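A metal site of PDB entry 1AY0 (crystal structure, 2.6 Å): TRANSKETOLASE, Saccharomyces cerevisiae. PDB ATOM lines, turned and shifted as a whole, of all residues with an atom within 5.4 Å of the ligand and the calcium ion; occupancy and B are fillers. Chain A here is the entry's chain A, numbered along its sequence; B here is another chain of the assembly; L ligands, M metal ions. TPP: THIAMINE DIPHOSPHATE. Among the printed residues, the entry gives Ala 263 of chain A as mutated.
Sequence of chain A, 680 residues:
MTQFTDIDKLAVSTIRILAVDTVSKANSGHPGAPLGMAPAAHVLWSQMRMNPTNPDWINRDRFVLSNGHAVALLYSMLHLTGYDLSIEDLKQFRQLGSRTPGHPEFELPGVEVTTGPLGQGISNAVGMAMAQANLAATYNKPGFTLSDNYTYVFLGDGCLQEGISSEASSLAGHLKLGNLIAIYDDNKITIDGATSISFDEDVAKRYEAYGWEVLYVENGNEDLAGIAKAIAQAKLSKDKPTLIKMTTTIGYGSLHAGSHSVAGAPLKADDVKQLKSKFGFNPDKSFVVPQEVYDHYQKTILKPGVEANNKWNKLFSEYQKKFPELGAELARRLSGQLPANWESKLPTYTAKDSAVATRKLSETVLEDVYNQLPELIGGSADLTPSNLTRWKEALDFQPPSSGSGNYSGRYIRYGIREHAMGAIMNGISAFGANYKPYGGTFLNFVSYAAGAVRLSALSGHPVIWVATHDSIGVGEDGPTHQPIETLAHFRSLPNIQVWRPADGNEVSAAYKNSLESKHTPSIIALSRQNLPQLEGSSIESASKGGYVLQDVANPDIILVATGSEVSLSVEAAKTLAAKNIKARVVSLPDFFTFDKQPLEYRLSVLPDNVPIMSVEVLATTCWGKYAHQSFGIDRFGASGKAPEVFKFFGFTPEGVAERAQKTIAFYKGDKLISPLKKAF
The backbone NH (N) of Asp 157 is in hydrogen-bond range of an oxygen (O2A) of the ligand (3.4 Å). NE2 of His 69 sits at hydrogen-bond distance from O1B of the ligand, at 2.7 Å. The backbone NH of Gly 158 is in hydrogen-bond range of an oxygen (O2A) of the ligand, at 2.9 Å. The backbone NH (N) of Leu 118 lies within hydrogen-bond range of a nitrogen (N3') of the ligand (3.2 Å). O of Gly 116 sits at hydrogen-bond distance from N4' of the ligand, at 3.3 Å.
The side-chain carboxylate of Asp 185 lies within hydrogen-bond range of the side-chain amide nitrogen of Asn 187, at 3.2 Å. OE1 of Glu 418 of chain B lies close to OE2 of Glu 162, at 2.5 Å. The side-chain carboxylate of Asp 382 of chain B is in hydrogen-bond range of the side-chain hydroxyl of Thr 190 (3.1 Å). The side-chain carboxylate (OD2) of Asp 382 of chain B sits close to the backbone NH (N) of Ile 191, 3.3 Å away. The backbone carbonyl oxygen of Leu 118 is in hydrogen-bond range of the side-chain hydroxyl of Tyr 448 of chain B (2.8 Å).
OE2 of Glu 418 of chain B sits close to N1' of the ligand (3.0 Å). Residues that only touch the ligand: Ala 33 (3.5 Å), Pro 117 (3.5 Å), Gly 156 (3.6 Å), Glu 162 (3.4 Å), Thr 190 (3.1 Å), Ile 191 (3.6 Å), Ile 250 (3.7 Å), Asp 382 of chain B (3.1 Å), Ile 416 of chain B (3.4 Å), Phe 445 of chain B (3.2 Å), Tyr 448 of chain B (3.4 Å) and His 481 of chain B (3.5 Å). Hydrophobic or aromatic side chains within 4 Å of the ligand: Ala 33, His 69, Leu 118, Ile 191, Ile 250, Ile 416 of chain B, Phe 445 of chain B and Tyr 448 of chain B. Of the 29 residues printed, 20 come within 4 Å of the ligand. Along chain A the residues within 4 Å of the ligand span positions 33 to 250.
The nearest printed residue that does not touch the calcium ion is Thr 190 (4.2 Å).
O3B of the ligand is bound to the calcium ion, 2.1 Å away. The side-chain amide oxygen (OD1) of Asn 187 is bound to the calcium ion, 2.3 Å away. OD2 of Asp 157 binds the calcium ion, 2.4 Å away. O of Ile 189 binds the calcium ion. The calcium ion is bound by an oxygen (O1A) of the ligand, at 2.7 Å. The calcium ion has five donor atoms within binding distance.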
ATOM      1  N   HIS A  30      20.730   2.062  -6.300  1.00  0.00           N
ATOM      2  CA  HIS A  30      19.846   3.110  -6.751  1.00  0.00           C
ATOM      3  C   HIS A  30      18.611   2.552  -7.388  1.00  0.00           C
ATOM      4  O   HIS A  30      18.677   2.042  -8.494  1.00  0.00           O
ATOM      5  CB  HIS A  30      20.563   3.977  -7.762  1.00  0.00           C
ATOM      6  CG  HIS A  30      21.823   4.587  -7.236  1.00  0.00           C
ATOM      7  ND1 HIS A  30      22.932   3.842  -6.894  1.00  0.00           N
ATOM      8  CD2 HIS A  30      22.143   5.878  -6.964  1.00  0.00           C
ATOM      9  CE1 HIS A  30      23.877   4.641  -6.443  1.00  0.00           C
ATOM     10  NE2 HIS A  30      23.426   5.886  -6.472  1.00  0.00           N
ATOM     11  N   ALA A  33      15.626   5.619 -10.518  1.00  0.00           N
ATOM     12  CA  ALA A  33      15.571   5.602 -11.981  1.00  0.00           C
ATOM     13  C   ALA A  33      15.142   4.253 -12.574  1.00  0.00           C
ATOM     14  O   ALA A  33      14.522   4.214 -13.628  1.00  0.00           O
ATOM     15  CB  ALA A  33      16.907   6.030 -12.535  1.00  0.00           C
ATOM     16  N   ASN A  67      23.397   7.043 -17.384  1.00  0.00           N
ATOM     17  CA  ASN A  67      23.110   7.172 -15.952  1.00  0.00           C
ATOM     18  C   ASN A  67      23.462   5.843 -15.296  1.00  0.00           C
ATOM     19  O   ASN A  67      22.599   5.155 -14.750  1.00  0.00           O
ATOM     20  CB  ASN A  67      21.646   7.570 -15.679  1.00  0.00           C
ATOM     21  CG  ASN A  67      20.637   6.844 -16.556  1.00  0.00           C
ATOM     22  OD1 ASN A  67      19.471   7.128 -16.490  1.00  0.00           O
ATOM     23  ND2 ASN A  67      21.083   5.899 -17.347  1.00  0.00           N
ATOM     24  N   HIS A  69      24.345   4.702 -12.574  1.00  0.00           N
ATOM     25  CA  HIS A  69      23.878   4.316 -11.266  1.00  0.00           C
ATOM     26  C   HIS A  69      22.618   3.485 -11.333  1.00  0.00           C
ATOM     27  O   HIS A  69      22.303   2.813 -10.382  1.00  0.00           O
ATOM     28  CB  HIS A  69      23.706   5.530 -10.332  1.00  0.00           C
ATOM     29  CG  HIS A  69      22.793   6.594 -10.849  1.00  0.00           C
ATOM     30  ND1 HIS A  69      23.215   7.589 -11.713  1.00  0.00           N
ATOM     31  CD2 HIS A  69      21.485   6.855 -10.608  1.00  0.00           C
ATOM     32  CE1 HIS A  69      22.211   8.399 -11.990  1.00  0.00           C
ATOM     33  NE2 HIS A  69      21.144   7.976 -11.328  1.00  0.00           N
ATOM     34  N   GLY A 116      29.290   5.107 -14.781  1.00  0.00           N
ATOM     35  CA  GLY A 116      29.149   5.349 -13.362  1.00  0.00           C
ATOM     36  C   GLY A 116      29.412   6.829 -13.236  1.00  0.00           C
ATOM     37  O   GLY A 116      28.595   7.577 -12.689  1.00  0.00           O
ATOM     38  N   PRO A 117      30.577   7.297 -13.694  1.00  0.00           N
ATOM     39  CA  PRO A 117      30.947   8.714 -13.650  1.00  0.00           C
ATOM     40  C   PRO A 117      30.012   9.429 -14.633  1.00  0.00           C
ATOM     41  O   PRO A 117      29.793   8.956 -15.771  1.00  0.00           O
ATOM     42  CB  PRO A 117      32.393   8.706 -14.151  1.00  0.00           C
ATOM     43  CG  PRO A 117      32.868   7.352 -13.670  1.00  0.00           C
ATOM     44  CD  PRO A 117      31.748   6.479 -14.088  1.00  0.00           C
ATOM     45  N   LEU A 118      29.485  10.578 -14.238  1.00  0.00           N
ATOM     46  CA  LEU A 118      28.531  11.259 -15.096  1.00  0.00           C
ATOM     47  C   LEU A 118      29.131  11.932 -16.299  1.00  0.00           C
ATOM     48  O   LEU A 118      30.264  12.418 -16.243  1.00  0.00           O
ATOM     49  CB  LEU A 118      27.650  12.215 -14.269  1.00  0.00           C
ATOM     50  CG  LEU A 118      26.859  11.538 -13.117  1.00  0.00           C
ATOM     51  CD1 LEU A 118      26.071  12.546 -12.334  1.00  0.00           C
ATOM     52  CD2 LEU A 118      25.942  10.436 -13.624  1.00  0.00           C
ATOM     53  N   GLY A 156      20.315  11.185 -17.686  1.00  0.00           N
ATOM     54  CA  GLY A 156      19.563  11.929 -16.681  1.00  0.00           C
ATOM     55  C   GLY A 156      20.107  13.338 -16.509  1.00  0.00           C
ATOM     56  O   GLY A 156      21.016  13.726 -17.240  1.00  0.00           O
ATOM     57  N   ASP A 157      19.608  14.081 -15.525  1.00  0.00           N
ATOM     58  CA  ASP A 157      20.029  15.470 -15.310  1.00  0.00           C
ATOM     59  C   ASP A 157      21.529  15.572 -15.088  1.00  0.00           C
ATOM     60  O   ASP A 157      22.163  16.482 -15.612  1.00  0.00           O
ATOM     61  CB  ASP A 157      19.299  16.086 -14.126  1.00  0.00           C
ATOM     62  CG  ASP A 157      17.794  15.932 -14.222  1.00  0.00           C
ATOM     63  OD1 ASP A 157      17.153  16.672 -14.985  1.00  0.00           O
ATOM     64  OD2 ASP A 157      17.229  15.071 -13.510  1.00  0.00           O
ATOM     65  N   GLY A 158      22.078  14.623 -14.358  1.00  0.00           N
ATOM     66  CA  GLY A 158      23.498  14.600 -14.081  1.00  0.00           C
ATOM     67  C   GLY A 158      24.390  14.674 -15.292  1.00  0.00           C
ATOM     68  O   GLY A 158      25.279  15.509 -15.353  1.00  0.00           O
ATOM     69  N   CYS A 159      24.212  13.769 -16.246  1.00  0.00           N
ATOM     70  CA  CYS A 159      25.022  13.792 -17.482  1.00  0.00           C
ATOM     71  C   CYS A 159      24.803  15.083 -18.273  1.00  0.00           C
ATOM     72  O   CYS A 159      25.692  15.501 -19.004  1.00  0.00           O
ATOM     73  CB  CYS A 159      24.696  12.598 -18.370  1.00  0.00           C
ATOM     74  SG  CYS A 159      24.918  11.064 -17.526  1.00  0.00           S
ATOM     75  N   GLU A 162      27.078  17.865 -16.627  1.00  0.00           N
ATOM     76  CA  GLU A 162      28.529  17.728 -16.827  1.00  0.00           C
ATOM     77  C   GLU A 162      28.972  18.249 -18.201  1.00  0.00           C
ATOM     78  O   GLU A 162      28.567  17.730 -19.230  1.00  0.00           O
ATOM     79  CB  GLU A 162      28.965  16.266 -16.693  1.00  0.00           C
ATOM     80  CG  GLU A 162      28.942  15.723 -15.278  1.00  0.00           C
ATOM     81  CD  GLU A 162      30.146  16.167 -14.439  1.00  0.00           C
ATOM     82  OE1 GLU A 162      30.941  17.042 -14.885  1.00  0.00           O
ATOM     83  OE2 GLU A 162      30.309  15.629 -13.327  1.00  0.00           O
ATOM     84  N   ASP A 185      15.805  11.009 -18.921  1.00  0.00           N
ATOM     85  CA  ASP A 185      14.922  10.773 -17.776  1.00  0.00           C
ATOM     86  C   ASP A 185      14.710  12.134 -17.074  1.00  0.00           C
ATOM     87  O   ASP A 185      15.475  12.548 -16.206  1.00  0.00           O
ATOM     88  CB  ASP A 185      15.597   9.761 -16.803  1.00  0.00           C
ATOM     89  CG  ASP A 185      14.654   9.290 -15.679  1.00  0.00           C
ATOM     90  OD1 ASP A 185      13.424   9.330 -15.863  1.00  0.00           O
ATOM     91  OD2 ASP A 185      15.131   8.843 -14.611  1.00  0.00           O
ATOM     92  N   ASN A 187      13.281  13.741 -14.543  1.00  0.00           N
ATOM     93  CA  ASN A 187      12.583  13.518 -13.286  1.00  0.00           C
ATOM     94  C   ASN A 187      12.558  14.603 -12.220  1.00  0.00           C
ATOM     95  O   ASN A 187      12.083  14.344 -11.109  1.00  0.00           O
ATOM     96  CB  ASN A 187      12.936  12.147 -12.678  1.00  0.00           C
ATOM     97  CG  ASN A 187      14.383  12.037 -12.223  1.00  0.00           C
ATOM     98  OD1 ASN A 187      15.059  13.035 -12.000  1.00  0.00           O
ATOM     99  ND2 ASN A 187      14.850  10.822 -12.072  1.00  0.00           N
ATOM    100  N   LYS A 188      13.097  15.780 -12.533  1.00  0.00           N
ATOM    101  CA  LYS A 188      13.061  16.924 -11.604  1.00  0.00           C
ATOM    102  C   LYS A 188      13.761  16.806 -10.249  1.00  0.00           C
ATOM    103  O   LYS A 188      13.570  17.634  -9.363  1.00  0.00           O
ATOM    104  CB  LYS A 188      11.591  17.292 -11.379  1.00  0.00           C
ATOM    105  CG  LYS A 188      11.050  18.354 -12.315  1.00  0.00           C
ATOM    106  CD  LYS A 188      10.759  17.893 -13.756  1.00  0.00           C
ATOM    107  CE  LYS A 188      10.441  19.122 -14.639  1.00  0.00           C
ATOM    108  NZ  LYS A 188      10.098  18.838 -16.051  1.00  0.00           N
ATOM    109  N   ILE A 189      14.669  15.838 -10.121  1.00  0.00           N
ATOM    110  CA  ILE A 189      15.333  15.601  -8.855  1.00  0.00           C
ATOM    111  C   ILE A 189      16.777  15.215  -9.099  1.00  0.00           C
ATOM    112  O   ILE A 189      17.119  14.751 -10.183  1.00  0.00           O
ATOM    113  CB  ILE A 189      14.602  14.421  -8.106  1.00  0.00           C
ATOM    114  CG1 ILE A 189      13.470  14.932  -7.229  1.00  0.00           C
ATOM    115  CG2 ILE A 189      15.562  13.574  -7.296  1.00  0.00           C
ATOM    116  CD1 ILE A 189      13.910  15.555  -5.917  1.00  0.00           C
ATOM    117  N   THR A 190      17.632  15.490  -8.112  1.00  0.00           N
ATOM    118  CA  THR A 190      19.045  15.118  -8.101  1.00  0.00           C
ATOM    119  C   THR A 190      19.406  15.015  -6.607  1.00  0.00           C
ATOM    120  O   THR A 190      18.575  15.351  -5.738  1.00  0.00           O
ATOM    121  CB  THR A 190      19.957  16.137  -8.819  1.00  0.00           C
ATOM    122  OG1 THR A 190      19.756  17.444  -8.269  1.00  0.00           O
ATOM    123  CG2 THR A 190      19.684  16.163 -10.309  1.00  0.00           C
ATOM    124  N   ILE A 191      20.624  14.555  -6.299  1.00  0.00           N
ATOM    125  CA  ILE A 191      21.035  14.380  -4.899  1.00  0.00           C
ATOM    126  C   ILE A 191      20.636  15.480  -3.917  1.00  0.00           C
ATOM    127  O   ILE A 191      19.890  15.227  -2.954  1.00  0.00           O
ATOM    128  CB  ILE A 191      22.560  14.075  -4.792  1.00  0.00           C
ATOM    129  CG1 ILE A 191      22.849  12.690  -5.337  1.00  0.00           C
ATOM    130  CG2 ILE A 191      23.036  14.105  -3.345  1.00  0.00           C
ATOM    131  CD1 ILE A 191      24.317  12.396  -5.416  1.00  0.00           C
ATOM    132  N   ILE A 250      10.571   9.795 -10.205  1.00  0.00           N
ATOM    133  CA  ILE A 250      11.615   8.972  -9.622  1.00  0.00           C
ATOM    134  C   ILE A 250      10.950   8.007  -8.647  1.00  0.00           C
ATOM    135  O   ILE A 250       9.958   8.375  -8.024  1.00  0.00           O
ATOM    136  CB  ILE A 250      12.707   9.849  -8.909  1.00  0.00           C
ATOM    137  CG1 ILE A 250      14.060   9.138  -8.895  1.00  0.00           C
ATOM    138  CG2 ILE A 250      12.310  10.162  -7.480  1.00  0.00           C
ATOM    139  CD1 ILE A 250      15.196   9.992  -8.333  1.00  0.00           C
ATOM    140  N   ALA A 263      16.346   7.961  -4.475  1.00  0.00           N
ATOM    141  CA  ALA A 263      17.339   8.124  -5.526  1.00  0.00           C
ATOM    142  C   ALA A 263      18.500   7.143  -5.462  1.00  0.00           C
ATOM    143  O   ALA A 263      18.716   6.385  -6.404  1.00  0.00           O
ATOM    144  CB  ALA A 263      17.849   9.553  -5.524  1.00  0.00           C
ATOM    145  N   ALA B 381      29.044  19.900  -4.916  1.00  0.00           N
ATOM    146  CA  ALA B 381      28.580  19.658  -6.273  1.00  0.00           C
ATOM    147  C   ALA B 381      27.573  18.528  -6.214  1.00  0.00           C
ATOM    148  O   ALA B 381      27.923  17.385  -6.499  1.00  0.00           O
ATOM    149  CB  ALA B 381      29.739  19.261  -7.167  1.00  0.00           C
ATOM    150  N   ASP B 382      26.340  18.825  -5.786  1.00  0.00           N
ATOM    151  CA  ASP B 382      25.256  17.831  -5.720  1.00  0.00           C
ATOM    152  C   ASP B 382      25.568  16.615  -4.835  1.00  0.00           C
ATOM    153  O   ASP B 382      25.093  15.509  -5.097  1.00  0.00           O
ATOM    154  CB  ASP B 382      24.883  17.363  -7.137  1.00  0.00           C
ATOM    155  CG  ASP B 382      23.563  16.630  -7.200  1.00  0.00           C
ATOM    156  OD1 ASP B 382      22.522  17.232  -6.878  1.00  0.00           O
ATOM    157  OD2 ASP B 382      23.546  15.454  -7.597  1.00  0.00           O
ATOM    158  N   LEU B 383      26.367  16.822  -3.799  1.00  0.00           N
ATOM    159  CA  LEU B 383      26.705  15.727  -2.909  1.00  0.00           C
ATOM    160  C   LEU B 383      26.659  16.182  -1.477  1.00  0.00           C
ATOM    161  O   LEU B 383      27.255  15.563  -0.599  1.00  0.00           O
ATOM    162  CB  LEU B 383      28.075  15.151  -3.252  1.00  0.00           C
ATOM    163  CG  LEU B 383      28.107  14.097  -4.363  1.00  0.00           C
ATOM    164  CD1 LEU B 383      29.516  13.875  -4.825  1.00  0.00           C
ATOM    165  CD2 LEU B 383      27.489  12.808  -3.878  1.00  0.00           C
ATOM    166  N   ILE B 416      26.074  19.122 -10.560  1.00  0.00           N
ATOM    167  CA  ILE B 416      27.100  18.144 -10.927  1.00  0.00           C
ATOM    168  C   ILE B 416      28.035  18.889 -11.903  1.00  0.00           C
ATOM    169  O   ILE B 416      27.989  18.679 -13.127  1.00  0.00           O
ATOM    170  CB  ILE B 416      26.475  16.900 -11.605  1.00  0.00           C
ATOM    171  CG1 ILE B 416      25.636  16.103 -10.607  1.00  0.00           C
ATOM    172  CG2 ILE B 416      27.526  15.983 -12.132  1.00  0.00           C
ATOM    173  CD1 ILE B 416      24.189  16.495 -10.560  1.00  0.00           C
ATOM    174  N   GLU B 418      31.880  19.707 -11.308  1.00  0.00           N
ATOM    175  CA  GLU B 418      33.152  19.786 -10.599  1.00  0.00           C
ATOM    176  C   GLU B 418      34.213  20.751 -11.140  1.00  0.00           C
ATOM    177  O   GLU B 418      34.866  21.449 -10.372  1.00  0.00           O
ATOM    178  CB  GLU B 418      33.751  18.413 -10.447  1.00  0.00           C
ATOM    179  CG  GLU B 418      32.868  17.457  -9.671  1.00  0.00           C
ATOM    180  CD  GLU B 418      31.804  16.766 -10.523  1.00  0.00           C
ATOM    181  OE1 GLU B 418      31.830  16.917 -11.765  1.00  0.00           O
ATOM    182  OE2 GLU B 418      30.946  16.053  -9.929  1.00  0.00           O
ATOM    183  N   PHE B 442      33.337  13.889  -4.348  1.00  0.00           N
ATOM    184  CA  PHE B 442      34.038  12.652  -4.060  1.00  0.00           C
ATOM    185  C   PHE B 442      35.475  12.781  -4.570  1.00  0.00           C
ATOM    186  O   PHE B 442      35.673  13.204  -5.711  1.00  0.00           O
ATOM    187  CB  PHE B 442      33.390  11.489  -4.812  1.00  0.00           C
ATOM    188  CG  PHE B 442      32.061  11.055  -4.247  1.00  0.00           C
ATOM    189  CD1 PHE B 442      31.766  11.217  -2.894  1.00  0.00           C
ATOM    190  CD2 PHE B 442      31.126  10.421  -5.073  1.00  0.00           C
ATOM    191  CE1 PHE B 442      30.543  10.764  -2.362  1.00  0.00           C
ATOM    192  CE2 PHE B 442      29.917   9.968  -4.569  1.00  0.00           C
ATOM    193  CZ  PHE B 442      29.613  10.140  -3.196  1.00  0.00           C
ATOM    194  N   PHE B 445      36.405  12.218  -8.074  1.00  0.00           N
ATOM    195  CA  PHE B 445      35.864  13.121  -9.078  1.00  0.00           C
ATOM    196  C   PHE B 445      36.520  14.490  -9.046  1.00  0.00           C
ATOM    197  O   PHE B 445      36.303  15.327  -9.912  1.00  0.00           O
ATOM    198  CB  PHE B 445      34.318  13.127  -9.043  1.00  0.00           C
ATOM    199  CG  PHE B 445      33.735  11.769  -9.411  1.00  0.00           C
ATOM    200  CD1 PHE B 445      34.245  11.046 -10.493  1.00  0.00           C
ATOM    201  CD2 PHE B 445      32.733  11.171  -8.620  1.00  0.00           C
ATOM    202  CE1 PHE B 445      33.786   9.755 -10.783  1.00  0.00           C
ATOM    203  CE2 PHE B 445      32.263   9.882  -8.902  1.00  0.00           C
ATOM    204  CZ  PHE B 445      32.785   9.164  -9.980  1.00  0.00           C
ATOM    205  N   TYR B 448      38.075  15.388 -12.176  1.00  0.00           N
ATOM    206  CA  TYR B 448      37.346  16.041 -13.261  1.00  0.00           C
ATOM    207  C   TYR B 448      37.698  17.532 -13.270  1.00  0.00           C
ATOM    208  O   TYR B 448      37.395  18.235 -14.218  1.00  0.00           O
ATOM    209  CB  TYR B 448      35.833  15.929 -13.022  1.00  0.00           C
ATOM    210  CG  TYR B 448      35.116  14.824 -13.727  1.00  0.00           C
ATOM    211  CD1 TYR B 448      35.583  13.527 -13.734  1.00  0.00           C
ATOM    212  CD2 TYR B 448      33.917  15.083 -14.364  1.00  0.00           C
ATOM    213  CE1 TYR B 448      34.863  12.500 -14.354  1.00  0.00           C
ATOM    214  CE2 TYR B 448      33.186  14.053 -14.997  1.00  0.00           C
ATOM    215  CZ  TYR B 448      33.671  12.778 -14.986  1.00  0.00           C
ATOM    216  OH  TYR B 448      32.935  11.797 -15.591  1.00  0.00           O
ATOM    217  N   HIS B 481      34.376   4.382  -8.695  1.00  0.00           N
ATOM    218  CA  HIS B 481      34.318   5.364  -7.612  1.00  0.00           C
ATOM    219  C   HIS B 481      35.407   5.297  -6.561  1.00  0.00           C
ATOM    220  O   HIS B 481      35.396   6.095  -5.644  1.00  0.00           O
ATOM    221  CB  HIS B 481      32.980   5.281  -6.897  1.00  0.00           C
ATOM    222  CG  HIS B 481      31.826   5.655  -7.764  1.00  0.00           C
ATOM    223  ND1 HIS B 481      31.633   5.125  -9.021  1.00  0.00           N
ATOM    224  CD2 HIS B 481      30.812   6.527  -7.558  1.00  0.00           C
ATOM    225  CE1 HIS B 481      30.552   5.655  -9.557  1.00  0.00           C
ATOM    226  NE2 HIS B 481      30.038   6.509  -8.692  1.00  0.00           N
HETATM  227  N1' TPP L   1      30.156  13.236 -10.542  1.00  0.00           N
HETATM  228  C2' TPP L   1      30.553  12.247 -11.350  1.00  0.00           C
HETATM  229  CM2 TPP L   1      31.410  12.568 -12.444  1.00  0.00           C
HETATM  230  N3' TPP L   1      30.200  11.012 -11.133  1.00  0.00           N
HETATM  231  C4' TPP L   1      29.244  10.755 -10.151  1.00  0.00           C
HETATM  232  N4' TPP L   1      28.859   9.539 -10.051  1.00  0.00           N
HETATM  233  C5' TPP L   1      28.842  11.743  -9.241  1.00  0.00           C
HETATM  234  C6' TPP L   1      29.304  12.990  -9.496  1.00  0.00           C
HETATM  235  C7' TPP L   1      27.958  11.452  -8.095  1.00  0.00           C
HETATM  236  N3  TPP L   1      26.586  11.277  -8.665  1.00  0.00           N
HETATM  237  C2  TPP L   1      25.993  10.075  -8.667  1.00  0.00           C
HETATM  238  S1  TPP L   1      24.323  10.181  -8.858  1.00  0.00           S
HETATM  239  C5  TPP L   1      24.462  11.861  -9.055  1.00  0.00           C
HETATM  240  C4  TPP L   1      25.745  12.275  -8.795  1.00  0.00           C
HETATM  241  CM4 TPP L   1      26.140  13.596  -8.348  1.00  0.00           C
HETATM  242  C6  TPP L   1      23.217  12.691  -8.955  1.00  0.00           C
HETATM  243  C7  TPP L   1      21.969  12.150  -9.601  1.00  0.00           C
HETATM  244  O7  TPP L   1      22.047  12.399 -11.013  1.00  0.00           O
HETATM  245  PA  TPP L   1      20.807  12.146 -11.910  1.00  0.00           P
HETATM  246  O1A TPP L   1      20.022  13.312 -11.555  1.00  0.00           O
HETATM  247  O2A TPP L   1      21.289  12.042 -13.339  1.00  0.00           O
HETATM  248  O3A TPP L   1      20.076  10.847 -11.346  1.00  0.00           O
HETATM  249  PB  TPP L   1      18.669  10.299 -10.868  1.00  0.00           P
HETATM  250  O1B TPP L   1      18.550   8.879 -11.234  1.00  0.00           O
HETATM  251  O2B TPP L   1      18.741  10.487  -9.415  1.00  0.00           O
HETATM  252  O3B TPP L   1      17.656  11.099 -11.584  1.00  0.00           O
HETATM  253 CA    CA M   1      17.349  13.149 -12.038  1.00  0.00          CA
